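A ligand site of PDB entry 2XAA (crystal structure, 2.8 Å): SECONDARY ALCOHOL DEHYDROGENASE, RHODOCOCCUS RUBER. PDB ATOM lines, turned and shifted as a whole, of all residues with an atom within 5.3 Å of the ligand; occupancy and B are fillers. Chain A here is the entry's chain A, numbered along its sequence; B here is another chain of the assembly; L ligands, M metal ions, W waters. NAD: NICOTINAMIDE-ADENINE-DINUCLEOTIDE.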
ATOM      1  N   CYS A  38     -20.947  -4.385  25.677  1.00  0.00           N
ATOM      2  CA  CYS A  38     -19.741  -5.104  26.106  1.00  0.00           C
ATOM      3  C   CYS A  38     -19.218  -4.504  27.418  1.00  0.00           C
ATOM      4  O   CYS A  38     -19.283  -3.273  27.618  1.00  0.00           O
ATOM      5  CB  CYS A  38     -18.635  -5.039  25.031  1.00  0.00           C
ATOM      6  SG  CYS A  38     -19.166  -5.170  23.254  1.00  0.00           S
ATOM      7  N   HIS A  39     -18.694  -5.371  28.275  1.00  0.00           N
ATOM      8  CA  HIS A  39     -18.040  -4.943  29.511  1.00  0.00           C
ATOM      9  C   HIS A  39     -17.000  -3.830  29.261  1.00  0.00           C
ATOM     10  O   HIS A  39     -16.731  -2.993  30.136  1.00  0.00           O
ATOM     11  CB  HIS A  39     -17.381  -6.132  30.196  1.00  0.00           C
ATOM     12  CG  HIS A  39     -17.108  -5.911  31.648  1.00  0.00           C
ATOM     13  ND1 HIS A  39     -17.890  -6.472  32.648  1.00  0.00           N
ATOM     14  CD2 HIS A  39     -16.146  -5.187  32.288  1.00  0.00           C
ATOM     15  CE1 HIS A  39     -17.424  -6.107  33.826  1.00  0.00           C
ATOM     16  NE2 HIS A  39     -16.365  -5.337  33.638  1.00  0.00           N
ATOM     17  N   SER A  40     -16.443  -3.820  28.042  1.00  0.00           N
ATOM     18  CA  SER A  40     -15.442  -2.837  27.628  1.00  0.00           C
ATOM     19  C   SER A  40     -15.936  -1.418  27.759  1.00  0.00           C
ATOM     20  O   SER A  40     -15.147  -0.526  28.064  1.00  0.00           O
ATOM     21  CB  SER A  40     -14.981  -3.109  26.192  1.00  0.00           C
ATOM     22  OG  SER A  40     -14.010  -4.137  26.149  1.00  0.00           O
ATOM     23  N   ASP A 153     -18.317  -9.611  18.466  1.00  0.00           N
ATOM     24  CA  ASP A 153     -17.275  -9.323  19.440  1.00  0.00           C
ATOM     25  C   ASP A 153     -17.169 -10.428  20.509  1.00  0.00           C
ATOM     26  O   ASP A 153     -16.094 -10.952  20.763  1.00  0.00           O
ATOM     27  CB  ASP A 153     -17.548  -7.924  20.032  1.00  0.00           C
ATOM     28  CG  ASP A 153     -16.602  -7.520  21.153  1.00  0.00           C
ATOM     29  OD1 ASP A 153     -15.523  -8.144  21.322  1.00  0.00           O
ATOM     30  OD2 ASP A 153     -16.964  -6.558  21.876  1.00  0.00           O
ATOM     31  N   THR A 157     -14.015 -12.143  19.205  1.00  0.00           N
ATOM     32  CA  THR A 157     -12.825 -12.054  20.049  1.00  0.00           C
ATOM     33  C   THR A 157     -12.313 -13.410  20.547  1.00  0.00           C
ATOM     34  O   THR A 157     -11.133 -13.696  20.451  1.00  0.00           O
ATOM     35  CB  THR A 157     -13.045 -11.133  21.229  1.00  0.00           C
ATOM     36  OG1 THR A 157     -13.017  -9.782  20.775  1.00  0.00           O
ATOM     37  CG2 THR A 157     -11.965 -11.308  22.263  1.00  0.00           C
ATOM     38  N   ILE A 178     -11.236 -19.439  31.486  1.00  0.00           N
ATOM     39  CA  ILE A 178     -11.423 -18.664  32.713  1.00  0.00           C
ATOM     40  C   ILE A 178     -12.334 -17.465  32.476  1.00  0.00           C
ATOM     41  O   ILE A 178     -11.986 -16.541  31.723  1.00  0.00           O
ATOM     42  CB  ILE A 178     -10.102 -18.141  33.391  1.00  0.00           C
ATOM     43  CG1 ILE A 178      -9.017 -19.220  33.524  1.00  0.00           C
ATOM     44  CG2 ILE A 178     -10.427 -17.645  34.791  1.00  0.00           C
ATOM     45  CD1 ILE A 178      -7.682 -18.730  34.227  1.00  0.00           C
ATOM     46  N   GLY A 179     -13.481 -17.501  33.140  1.00  0.00           N
ATOM     47  CA  GLY A 179     -14.467 -16.440  33.090  1.00  0.00           C
ATOM     48  C   GLY A 179     -15.540 -16.867  32.140  1.00  0.00           C
ATOM     49  O   GLY A 179     -15.413 -16.633  30.946  1.00  0.00           O
ATOM     50  N   VAL A 180     -16.584 -17.509  32.643  1.00  0.00           N
ATOM     51  CA  VAL A 180     -17.668 -17.975  31.779  1.00  0.00           C
ATOM     52  C   VAL A 180     -18.716 -16.851  31.570  1.00  0.00           C
ATOM     53  O   VAL A 180     -19.918 -17.044  31.781  1.00  0.00           O
ATOM     54  CB  VAL A 180     -18.307 -19.281  32.330  1.00  0.00           C
ATOM     55  CG1 VAL A 180     -19.302 -19.870  31.346  1.00  0.00           C
ATOM     56  CG2 VAL A 180     -17.272 -20.321  32.639  1.00  0.00           C
ATOM     57  N   GLY A 181     -18.255 -15.668  31.137  1.00  0.00           N
ATOM     58  CA  GLY A 181     -19.122 -14.506  31.000  1.00  0.00           C
ATOM     59  C   GLY A 181     -19.791 -14.404  29.658  1.00  0.00           C
ATOM     60  O   GLY A 181     -20.147 -15.413  29.079  1.00  0.00           O
ATOM     61  N   GLY A 182     -19.974 -13.180  29.170  1.00  0.00           N
ATOM     62  CA  GLY A 182     -20.546 -12.973  27.857  1.00  0.00           C
ATOM     63  C   GLY A 182     -19.632 -13.647  26.849  1.00  0.00           C
ATOM     64  O   GLY A 182     -20.069 -14.509  26.088  1.00  0.00           O
ATOM     65  N   LEU A 183     -18.353 -13.272  26.861  1.00  0.00           N
ATOM     66  CA  LEU A 183     -17.334 -13.880  26.002  1.00  0.00           C
ATOM     67  C   LEU A 183     -17.091 -15.340  26.373  1.00  0.00           C
ATOM     68  O   LEU A 183     -17.240 -16.224  25.533  1.00  0.00           O
ATOM     69  CB  LEU A 183     -16.036 -13.121  26.139  1.00  0.00           C
ATOM     70  CG  LEU A 183     -15.715 -12.025  25.142  1.00  0.00           C
ATOM     71  CD1 LEU A 183     -16.687 -10.881  25.177  1.00  0.00           C
ATOM     72  CD2 LEU A 183     -14.334 -11.569  25.511  1.00  0.00           C
ATOM     73  N   GLY A 184     -16.714 -15.582  27.632  1.00  0.00           N
ATOM     74  CA  GLY A 184     -16.432 -16.944  28.098  1.00  0.00           C
ATOM     75  C   GLY A 184     -17.352 -17.998  27.485  1.00  0.00           C
ATOM     76  O   GLY A 184     -16.884 -18.934  26.841  1.00  0.00           O
ATOM     77  N   VAL A 202     -13.680 -22.261  34.399  1.00  0.00           N
ATOM     78  CA  VAL A 202     -13.397 -21.748  35.762  1.00  0.00           C
ATOM     79  C   VAL A 202     -14.192 -20.481  35.919  1.00  0.00           C
ATOM     80  O   VAL A 202     -14.394 -19.774  34.927  1.00  0.00           O
ATOM     81  CB  VAL A 202     -11.891 -21.426  35.957  1.00  0.00           C
ATOM     82  CG1 VAL A 202     -11.594 -20.894  37.358  1.00  0.00           C
ATOM     83  CG2 VAL A 202     -11.024 -22.644  35.635  1.00  0.00           C
ATOM     84  N   ASP A 203     -14.662 -20.205  37.142  1.00  0.00           N
ATOM     85  CA  ASP A 203     -15.454 -18.988  37.468  1.00  0.00           C
ATOM     86  C   ASP A 203     -15.659 -18.833  38.965  1.00  0.00           C
ATOM     87  O   ASP A 203     -15.672 -19.809  39.704  1.00  0.00           O
ATOM     88  CB  ASP A 203     -16.822 -18.981  36.759  1.00  0.00           C
ATOM     89  CG  ASP A 203     -17.392 -17.586  36.601  1.00  0.00           C
ATOM     90  OD1 ASP A 203     -17.655 -17.169  35.431  1.00  0.00           O
ATOM     91  OD2 ASP A 203     -17.561 -16.887  37.634  1.00  0.00           O
ATOM     92  N   LEU A 204     -15.815 -17.595  39.398  1.00  0.00           N
ATOM     93  CA  LEU A 204     -16.150 -17.311  40.787  1.00  0.00           C
ATOM     94  C   LEU A 204     -17.570 -17.762  41.169  1.00  0.00           C
ATOM     95  O   LEU A 204     -17.793 -18.222  42.298  1.00  0.00           O
ATOM     96  CB  LEU A 204     -16.031 -15.801  41.075  1.00  0.00           C
ATOM     97  CG  LEU A 204     -14.673 -15.109  41.142  1.00  0.00           C
ATOM     98  CD1 LEU A 204     -14.868 -13.618  41.214  1.00  0.00           C
ATOM     99  CD2 LEU A 204     -13.835 -15.590  42.337  1.00  0.00           C
ATOM    100  N   ASP A 205     -18.518 -17.622  40.244  1.00  0.00           N
ATOM    101  CA  ASP A 205     -19.944 -17.807  40.534  1.00  0.00           C
ATOM    102  C   ASP A 205     -20.497 -19.200  40.099  1.00  0.00           C
ATOM    103  O   ASP A 205     -20.337 -19.628  38.951  1.00  0.00           O
ATOM    104  CB  ASP A 205     -20.746 -16.599  39.997  1.00  0.00           C
ATOM    105  CG  ASP A 205     -22.210 -16.910  39.687  1.00  0.00           C
ATOM    106  OD1 ASP A 205     -22.496 -17.860  38.945  1.00  0.00           O
ATOM    107  OD2 ASP A 205     -23.073 -16.146  40.145  1.00  0.00           O
ATOM    108  N   ARG A 208     -22.703 -19.554  36.932  1.00  0.00           N
ATOM    109  CA  ARG A 208     -21.848 -19.462  35.722  1.00  0.00           C
ATOM    110  C   ARG A 208     -21.172 -20.778  35.356  1.00  0.00           C
ATOM    111  O   ARG A 208     -21.017 -21.107  34.178  1.00  0.00           O
ATOM    112  CB  ARG A 208     -20.806 -18.336  35.882  1.00  0.00           C
ATOM    113  CG  ARG A 208     -21.365 -16.935  35.947  1.00  0.00           C
ATOM    114  CD  ARG A 208     -22.453 -16.652  34.885  1.00  0.00           C
ATOM    115  NE  ARG A 208     -23.080 -15.364  35.190  1.00  0.00           N
ATOM    116  CZ  ARG A 208     -22.806 -14.219  34.562  1.00  0.00           C
ATOM    117  NH1 ARG A 208     -21.963 -14.193  33.528  1.00  0.00           N
ATOM    118  NH2 ARG A 208     -23.396 -13.091  34.935  1.00  0.00           N
ATOM    119  N   SER A 223     -13.272 -20.823  40.895  1.00  0.00           N
ATOM    120  CA  SER A 223     -12.175 -19.885  40.827  1.00  0.00           C
ATOM    121  C   SER A 223     -11.657 -19.596  42.226  1.00  0.00           C
ATOM    122  O   SER A 223     -12.428 -19.600  43.187  1.00  0.00           O
ATOM    123  CB  SER A 223     -12.656 -18.601  40.184  1.00  0.00           C
ATOM    124  OG  SER A 223     -11.615 -18.006  39.465  1.00  0.00           O
ATOM    125  N   PHE A 246     -10.426 -14.902  30.251  1.00  0.00           N
ATOM    126  CA  PHE A 246     -11.339 -13.839  29.829  1.00  0.00           C
ATOM    127  C   PHE A 246     -11.593 -12.850  30.927  1.00  0.00           C
ATOM    128  O   PHE A 246     -12.479 -12.014  30.817  1.00  0.00           O
ATOM    129  CB  PHE A 246     -12.649 -14.409  29.316  1.00  0.00           C
ATOM    130  CG  PHE A 246     -12.460 -15.273  28.120  1.00  0.00           C
ATOM    131  CD1 PHE A 246     -12.227 -14.704  26.863  1.00  0.00           C
ATOM    132  CD2 PHE A 246     -12.471 -16.666  28.243  1.00  0.00           C
ATOM    133  CE1 PHE A 246     -12.038 -15.515  25.725  1.00  0.00           C
ATOM    134  CE2 PHE A 246     -12.302 -17.468  27.140  1.00  0.00           C
ATOM    135  CZ  PHE A 246     -12.088 -16.902  25.870  1.00  0.00           C
ATOM    136  N   VAL A 247     -10.789 -12.949  31.989  1.00  0.00           N
ATOM    137  CA  VAL A 247     -10.954 -12.091  33.138  1.00  0.00           C
ATOM    138  C   VAL A 247      -9.747 -11.196  33.133  1.00  0.00           C
ATOM    139  O   VAL A 247      -9.868  -9.968  33.204  1.00  0.00           O
ATOM    140  CB  VAL A 247     -11.044 -12.884  34.459  1.00  0.00           C
ATOM    141  CG1 VAL A 247     -11.043 -11.953  35.633  1.00  0.00           C
ATOM    142  CG2 VAL A 247     -12.309 -13.801  34.496  1.00  0.00           C
ATOM    143  N   SER A 251      -4.855 -12.363  39.572  1.00  0.00           N
ATOM    144  CA  SER A 251      -5.080 -13.682  40.191  1.00  0.00           C
ATOM    145  C   SER A 251      -5.390 -14.763  39.139  1.00  0.00           C
ATOM    146  O   SER A 251      -4.950 -15.910  39.294  1.00  0.00           O
ATOM    147  CB  SER A 251      -6.116 -13.644  41.332  1.00  0.00           C
ATOM    148  OG  SER A 251      -7.422 -13.945  40.857  1.00  0.00           O
ATOM    149  N   THR A 252      -6.101 -14.415  38.066  1.00  0.00           N
ATOM    150  CA  THR A 252      -6.438 -15.382  37.042  1.00  0.00           C
ATOM    151  C   THR A 252      -5.180 -15.699  36.229  1.00  0.00           C
ATOM    152  O   THR A 252      -4.893 -16.869  35.909  1.00  0.00           O
ATOM    153  CB  THR A 252      -7.573 -14.891  36.102  1.00  0.00           C
ATOM    154  OG1 THR A 252      -7.244 -13.612  35.516  1.00  0.00           O
ATOM    155  CG2 THR A 252      -8.919 -14.827  36.844  1.00  0.00           C
ATOM    156  N   VAL A 268      -4.324 -13.950  27.191  1.00  0.00           N
ATOM    157  CA  VAL A 268      -4.845 -12.990  28.150  1.00  0.00           C
ATOM    158  C   VAL A 268      -5.804 -12.059  27.442  1.00  0.00           C
ATOM    159  O   VAL A 268      -5.413 -11.102  26.746  1.00  0.00           O
ATOM    160  CB  VAL A 268      -3.710 -12.252  28.809  1.00  0.00           C
ATOM    161  CG1 VAL A 268      -4.213 -11.053  29.637  1.00  0.00           C
ATOM    162  CG2 VAL A 268      -2.965 -13.212  29.702  1.00  0.00           C
ATOM    163  N   VAL A 269      -7.086 -12.332  27.627  1.00  0.00           N
ATOM    164  CA  VAL A 269      -8.106 -11.715  26.809  1.00  0.00           C
ATOM    165  C   VAL A 269      -8.928 -10.687  27.569  1.00  0.00           C
ATOM    166  O   VAL A 269      -9.461  -9.760  26.959  1.00  0.00           O
ATOM    167  CB  VAL A 269      -9.027 -12.779  26.253  1.00  0.00           C
ATOM    168  CG1 VAL A 269     -10.034 -12.162  25.394  1.00  0.00           C
ATOM    169  CG2 VAL A 269      -8.192 -13.804  25.498  1.00  0.00           C
ATOM    170  N   GLY A 270      -9.046 -10.867  28.886  1.00  0.00           N
ATOM    171  CA  GLY A 270      -9.749  -9.909  29.750  1.00  0.00           C
ATOM    172  C   GLY A 270      -8.853  -8.747  30.128  1.00  0.00           C
ATOM    173  O   GLY A 270      -7.624  -8.903  30.213  1.00  0.00           O
ATOM    174  N   ILE A 271      -9.448  -7.575  30.367  1.00  0.00           N
ATOM    175  CA  ILE A 271      -8.659  -6.382  30.702  1.00  0.00           C
ATOM    176  C   ILE A 271      -8.763  -5.928  32.150  1.00  0.00           C
ATOM    177  O   ILE A 271      -9.805  -5.440  32.574  1.00  0.00           O
ATOM    178  CB  ILE A 271      -8.991  -5.213  29.746  1.00  0.00           C
ATOM    179  CG1 ILE A 271      -8.942  -5.723  28.292  1.00  0.00           C
ATOM    180  CG2 ILE A 271      -8.045  -4.005  30.006  1.00  0.00           C
ATOM    181  CD1 ILE A 271      -9.351  -4.730  27.204  1.00  0.00           C
ATOM    182  N   PRO A 293      -4.438 -10.857  22.814  1.00  0.00           N
ATOM    183  CA  PRO A 293      -4.985 -10.690  21.475  1.00  0.00           C
ATOM    184  C   PRO A 293      -5.976  -9.528  21.441  1.00  0.00           C
ATOM    185  O   PRO A 293      -6.566  -9.216  22.446  1.00  0.00           O
ATOM    186  CB  PRO A 293      -5.681 -12.031  21.234  1.00  0.00           C
ATOM    187  CG  PRO A 293      -6.030 -12.511  22.580  1.00  0.00           C
ATOM    188  CD  PRO A 293      -5.107 -11.912  23.569  1.00  0.00           C
ATOM    189  N   TYR A 294      -6.157  -8.892  20.287  1.00  0.00           N
ATOM    190  CA  TYR A 294      -7.178  -7.855  20.199  1.00  0.00           C
ATOM    191  C   TYR A 294      -8.256  -8.151  19.153  1.00  0.00           C
ATOM    192  O   TYR A 294      -7.948  -8.429  17.984  1.00  0.00           O
ATOM    193  CB  TYR A 294      -6.541  -6.494  19.993  1.00  0.00           C
ATOM    194  CG  TYR A 294      -7.483  -5.415  19.484  1.00  0.00           C
ATOM    195  CD1 TYR A 294      -8.502  -4.904  20.296  1.00  0.00           C
ATOM    196  CD2 TYR A 294      -7.335  -4.876  18.205  1.00  0.00           C
ATOM    197  CE1 TYR A 294      -9.359  -3.893  19.831  1.00  0.00           C
ATOM    198  CE2 TYR A 294      -8.192  -3.864  17.740  1.00  0.00           C
ATOM    199  CZ  TYR A 294      -9.199  -3.382  18.556  1.00  0.00           C
ATOM    200  OH  TYR A 294     -10.033  -2.387  18.100  1.00  0.00           O
ATOM    201  N   TRP A 295      -9.514  -8.084  19.595  1.00  0.00           N
ATOM    202  CA  TRP A 295     -10.671  -8.224  18.732  1.00  0.00           C
ATOM    203  C   TRP A 295     -10.453  -9.331  17.709  1.00  0.00           C
ATOM    204  O   TRP A 295     -10.027 -10.418  18.101  1.00  0.00           O
ATOM    205  CB  TRP A 295     -11.021  -6.875  18.110  1.00  0.00           C
ATOM    206  CG  TRP A 295     -12.497  -6.635  18.003  1.00  0.00           C
ATOM    207  CD1 TRP A 295     -13.512  -7.595  17.900  1.00  0.00           C
ATOM    208  CD2 TRP A 295     -13.164  -5.370  17.952  1.00  0.00           C
ATOM    209  NE1 TRP A 295     -14.732  -6.973  17.820  1.00  0.00           N
ATOM    210  CE2 TRP A 295     -14.545  -5.606  17.827  1.00  0.00           C
ATOM    211  CE3 TRP A 295     -12.723  -4.045  18.002  1.00  0.00           C
ATOM    212  CZ2 TRP A 295     -15.471  -4.577  17.754  1.00  0.00           C
ATOM    213  CZ3 TRP A 295     -13.644  -3.035  17.925  1.00  0.00           C
ATOM    214  CH2 TRP A 295     -15.000  -3.306  17.798  1.00  0.00           C
ATOM    215  N   LEU A 332     -24.802  -5.080  34.082  1.00  0.00           N
ATOM    216  CA  LEU A 332     -23.500  -5.589  33.594  1.00  0.00           C
ATOM    217  C   LEU A 332     -22.406  -5.411  34.675  1.00  0.00           C
ATOM    218  O   LEU A 332     -21.823  -6.407  35.154  1.00  0.00           O
ATOM    219  CB  LEU A 332     -23.080  -4.914  32.271  1.00  0.00           C
ATOM    220  N   GLY A 339     -24.961 -14.255  30.381  1.00  0.00           N
ATOM    221  CA  GLY A 339     -24.599 -14.188  28.951  1.00  0.00           C
ATOM    222  C   GLY A 339     -24.422 -12.738  28.532  1.00  0.00           C
ATOM    223  O   GLY A 339     -23.942 -11.944  29.325  1.00  0.00           O
ATOM    224  N   ARG A 340     -24.816 -12.402  27.307  1.00  0.00           N
ATOM    225  CA  ARG A 340     -24.713 -11.004  26.825  1.00  0.00           C
ATOM    226  C   ARG A 340     -25.912 -10.188  27.228  1.00  0.00           C
ATOM    227  O   ARG A 340     -26.754 -10.665  27.954  1.00  0.00           O
ATOM    228  CB  ARG A 340     -24.564 -10.914  25.284  1.00  0.00           C
ATOM    229  CG  ARG A 340     -23.169 -10.497  24.766  1.00  0.00           C
ATOM    230  CD  ARG A 340     -22.808  -9.054  25.033  1.00  0.00           C
ATOM    231  NE  ARG A 340     -21.399  -8.778  24.733  1.00  0.00           N
ATOM    232  CZ  ARG A 340     -20.379  -9.079  25.546  1.00  0.00           C
ATOM    233  NH1 ARG A 340     -20.569  -9.685  26.722  1.00  0.00           N
ATOM    234  NH2 ARG A 340     -19.140  -8.777  25.191  1.00  0.00           N
ATOM    235  N   PHE B 281      -2.251  -5.814  28.869  1.00  0.00           N
ATOM    236  CA  PHE B 281      -2.743  -4.714  28.057  1.00  0.00           C
ATOM    237  C   PHE B 281      -2.057  -3.416  28.473  1.00  0.00           C
ATOM    238  O   PHE B 281      -1.835  -3.188  29.680  1.00  0.00           O
ATOM    239  CB  PHE B 281      -4.271  -4.628  28.146  1.00  0.00           C
ATOM    240  CG  PHE B 281      -4.974  -5.750  27.423  1.00  0.00           C
ATOM    241  CD1 PHE B 281      -5.414  -6.864  28.096  1.00  0.00           C
ATOM    242  CD2 PHE B 281      -5.172  -5.689  26.038  1.00  0.00           C
ATOM    243  CE1 PHE B 281      -6.035  -7.909  27.422  1.00  0.00           C
ATOM    244  CE2 PHE B 281      -5.799  -6.698  25.333  1.00  0.00           C
ATOM    245  CZ  PHE B 281      -6.235  -7.812  26.016  1.00  0.00           C
HETATM  246  PA  NAD L   1     -18.834 -10.492  31.559  1.00  0.00           P
HETATM  247  O1A NAD L   1     -19.045  -9.586  32.722  1.00  0.00           O
HETATM  248  O2A NAD L   1     -20.005 -10.681  30.658  1.00  0.00           O
HETATM  249  O5B NAD L   1     -18.342 -11.883  32.171  1.00  0.00           O
HETATM  250  C5B NAD L   1     -17.733 -11.891  33.423  1.00  0.00           C
HETATM  251  C4B NAD L   1     -17.636 -13.305  33.954  1.00  0.00           C
HETATM  252  O4B NAD L   1     -16.367 -13.425  34.555  1.00  0.00           O
HETATM  253  C3B NAD L   1     -18.681 -13.550  35.014  1.00  0.00           C
HETATM  254  O3B NAD L   1     -19.277 -14.814  34.789  1.00  0.00           O
HETATM  255  C2B NAD L   1     -17.906 -13.520  36.312  1.00  0.00           C
HETATM  256  O2B NAD L   1     -18.445 -14.434  37.250  1.00  0.00           O
HETATM  257  C1B NAD L   1     -16.528 -13.949  35.842  1.00  0.00           C
HETATM  258  N9A NAD L   1     -15.405 -13.495  36.661  1.00  0.00           N
HETATM  259  C8A NAD L   1     -15.085 -12.229  37.152  1.00  0.00           C
HETATM  260  N7A NAD L   1     -13.941 -12.379  37.901  1.00  0.00           N
HETATM  261  C5A NAD L   1     -13.543 -13.696  37.882  1.00  0.00           C
HETATM  262  C6A NAD L   1     -12.481 -14.424  38.434  1.00  0.00           C
HETATM  263  N6A NAD L   1     -11.727 -13.888  39.401  1.00  0.00           N
HETATM  264  N1A NAD L   1     -12.364 -15.795  38.214  1.00  0.00           N
HETATM  265  C2A NAD L   1     -13.292 -16.448  37.465  1.00  0.00           C
HETATM  266  N3A NAD L   1     -14.349 -15.752  36.921  1.00  0.00           N
HETATM  267  C4A NAD L   1     -14.462 -14.397  37.116  1.00  0.00           C
HETATM  268  O3  NAD L   1     -17.582  -9.911  30.713  1.00  0.00           O
HETATM  269  PN  NAD L   1     -17.451 -10.056  29.108  1.00  0.00           P
HETATM  270  O1N NAD L   1     -18.112  -8.927  28.401  1.00  0.00           O
HETATM  271  O2N NAD L   1     -17.805 -11.444  28.713  1.00  0.00           O
HETATM  272  O5D NAD L   1     -15.856  -9.870  28.954  1.00  0.00           O
HETATM  273  C5D NAD L   1     -14.876 -10.373  29.842  1.00  0.00           C
HETATM  274  C4D NAD L   1     -13.584  -9.559  29.652  1.00  0.00           C
HETATM  275  O4D NAD L   1     -13.187  -9.629  28.280  1.00  0.00           O
HETATM  276  C3D NAD L   1     -13.744  -8.063  29.990  1.00  0.00           C
HETATM  277  O3D NAD L   1     -12.676  -7.576  30.772  1.00  0.00           O
HETATM  278  C2D NAD L   1     -13.755  -7.394  28.619  1.00  0.00           C
HETATM  279  O2D NAD L   1     -13.168  -6.140  28.644  1.00  0.00           O
HETATM  280  C1D NAD L   1     -12.864  -8.320  27.812  1.00  0.00           C
HETATM  281  N1N NAD L   1     -12.888  -8.058  26.335  1.00  0.00           N
HETATM  282  C2N NAD L   1     -11.672  -7.953  25.692  1.00  0.00           C
HETATM  283  C3N NAD L   1     -11.565  -7.703  24.315  1.00  0.00           C
HETATM  284  C7N NAD L   1     -10.235  -7.907  23.625  1.00  0.00           C
HETATM  285  O7N NAD L   1     -10.035  -7.306  22.375  1.00  0.00           O
HETATM  286  N7N NAD L   1      -9.302  -8.637  24.225  1.00  0.00           N
HETATM  287  C4N NAD L   1     -12.721  -7.544  23.550  1.00  0.00           C
HETATM  288  C5N NAD L   1     -13.956  -7.648  24.226  1.00  0.00           C
HETATM  289  C6N NAD L   1     -14.038  -7.902  25.601  1.00  0.00           C
HETATM  290 ZN    ZN M   1     -15.954  -5.482  23.467  1.00  0.00          ZN
HETATM  291  O   HOH W   1     -12.838  -4.456  22.987  1.00  0.00           O
HETATM  292  O   HOH W   2     -16.460 -13.768  29.816  1.00  0.00           O
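The side-chain carboxylate (OD2) of Asp 203 sits at hydrogen-bond distance from an oxygen (O2B) of the ligand, at 2.6 Å.
N1A of the ligand is in hydrogen-bond range of OG of Ser 223, at 2.6 Å.
An oxygen (O2N) of the ligand sits at hydrogen-bond distance from the backbone NH (N) of Leu 183 (2.7 Å).
N of Gly 182 sits at hydrogen-bond distance from O2N of the ligand.
The backbone NH (N) of Trp 295 is in hydrogen-bond range of an oxygen (O7N) of the ligand.
The backbone carbonyl oxygen of Val 269 lies within hydrogen-bond range of a nitrogen (N7N) of the ligand (3.0 Å).
O3B of the ligand is in hydrogen-bond range of NH1 of Arg 208, 3.0 Å away.
An oxygen (O1N) of the ligand lies within salt-bridge range of the guanidinium group (NH1) of Arg 340.
The backbone NH (N) of Ile 271 is in hydrogen-bond range of an oxygen (O3D) of the ligand, at 3.3 Å.
OG of Ser 40 is in hydrogen-bond range of O2D of the ligand, at 3.3 Å.
A nitrogen (N7N) of the ligand sits at hydrogen-bond distance from the backbone carbonyl oxygen (O) of Pro 293, 3.3 Å away.
A ring nitrogen (ND1) of His 39 is in hydrogen-bond range of an oxygen (O1A) of the ligand.
The backbone NH (N) of Leu 204 lies close to a nitrogen (N3A) of the ligand, 3.4 Å away.
The backbone carbonyl oxygen of Asp 203 sits at hydrogen-bond distance from the backbone NH of Ser 223 (2.9 Å).
N of Val 180 sits at hydrogen-bond distance from OD1 of Asp 203, at 3.0 Å.
N of Asp 205 sits at hydrogen-bond distance from OD2 of Asp 203 (2.9 Å).
The backbone NH (N) of Phe 246 lies within hydrogen-bond range of the backbone carbonyl oxygen (O) of Ile 178, at 2.7 Å.
The backbone NH of Arg 208 is in hydrogen-bond range of the side-chain carboxylate of Asp 205.
OD1 of Asp 153 lies within hydrogen-bond range of OG1 of Thr 157 (3.0 Å).
The side-chain carboxylate (OD2) of Asp 153 lies close to the side-chain sulfur (SG) of Cys 38, 2.9 Å away.
The backbone carbonyl oxygen of Val 202 sits at hydrogen-bond distance from the backbone NH of Gly 179 (3.0 Å).
OD1 of Asp 153 touches C5N of the ligand, at 3.3 Å.
Thr 157 touches the ligand (OG1 to C4N, 3.6 Å).
CA of Gly 179 touches O4B of the ligand, at 3.9 Å.
Val 180 touches the ligand (O to O3B, 3.8 Å).
Gly 181 touches the ligand (CA to O5B, 3.0 Å).
O of Phe 246 touches C4D of the ligand, 2.9 Å away.
Val 247 touches the ligand (CG2 to C4A, 3.4 Å).
CG2 of Thr 252 touches N1A of the ligand (3.8 Å).
CA of Gly 270 touches O4D of the ligand, at 3.7 Å.
Tyr 294 touches the ligand (CD1 to O7N, 3.5 Å).
Phe 281 of chain B touches the ligand (CZ to N7N, 3.6 Å).
Water W2 lies within hydrogen-bond range of the backbone NH (N) of Gly 184 (2.9 Å), an oxygen (O2N) of the ligand (2.9 Å), the backbone NH (N) of Gly 181 (2.9 Å) and the backbone carbonyl oxygen (O) of Gly 179 (3.3 Å).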
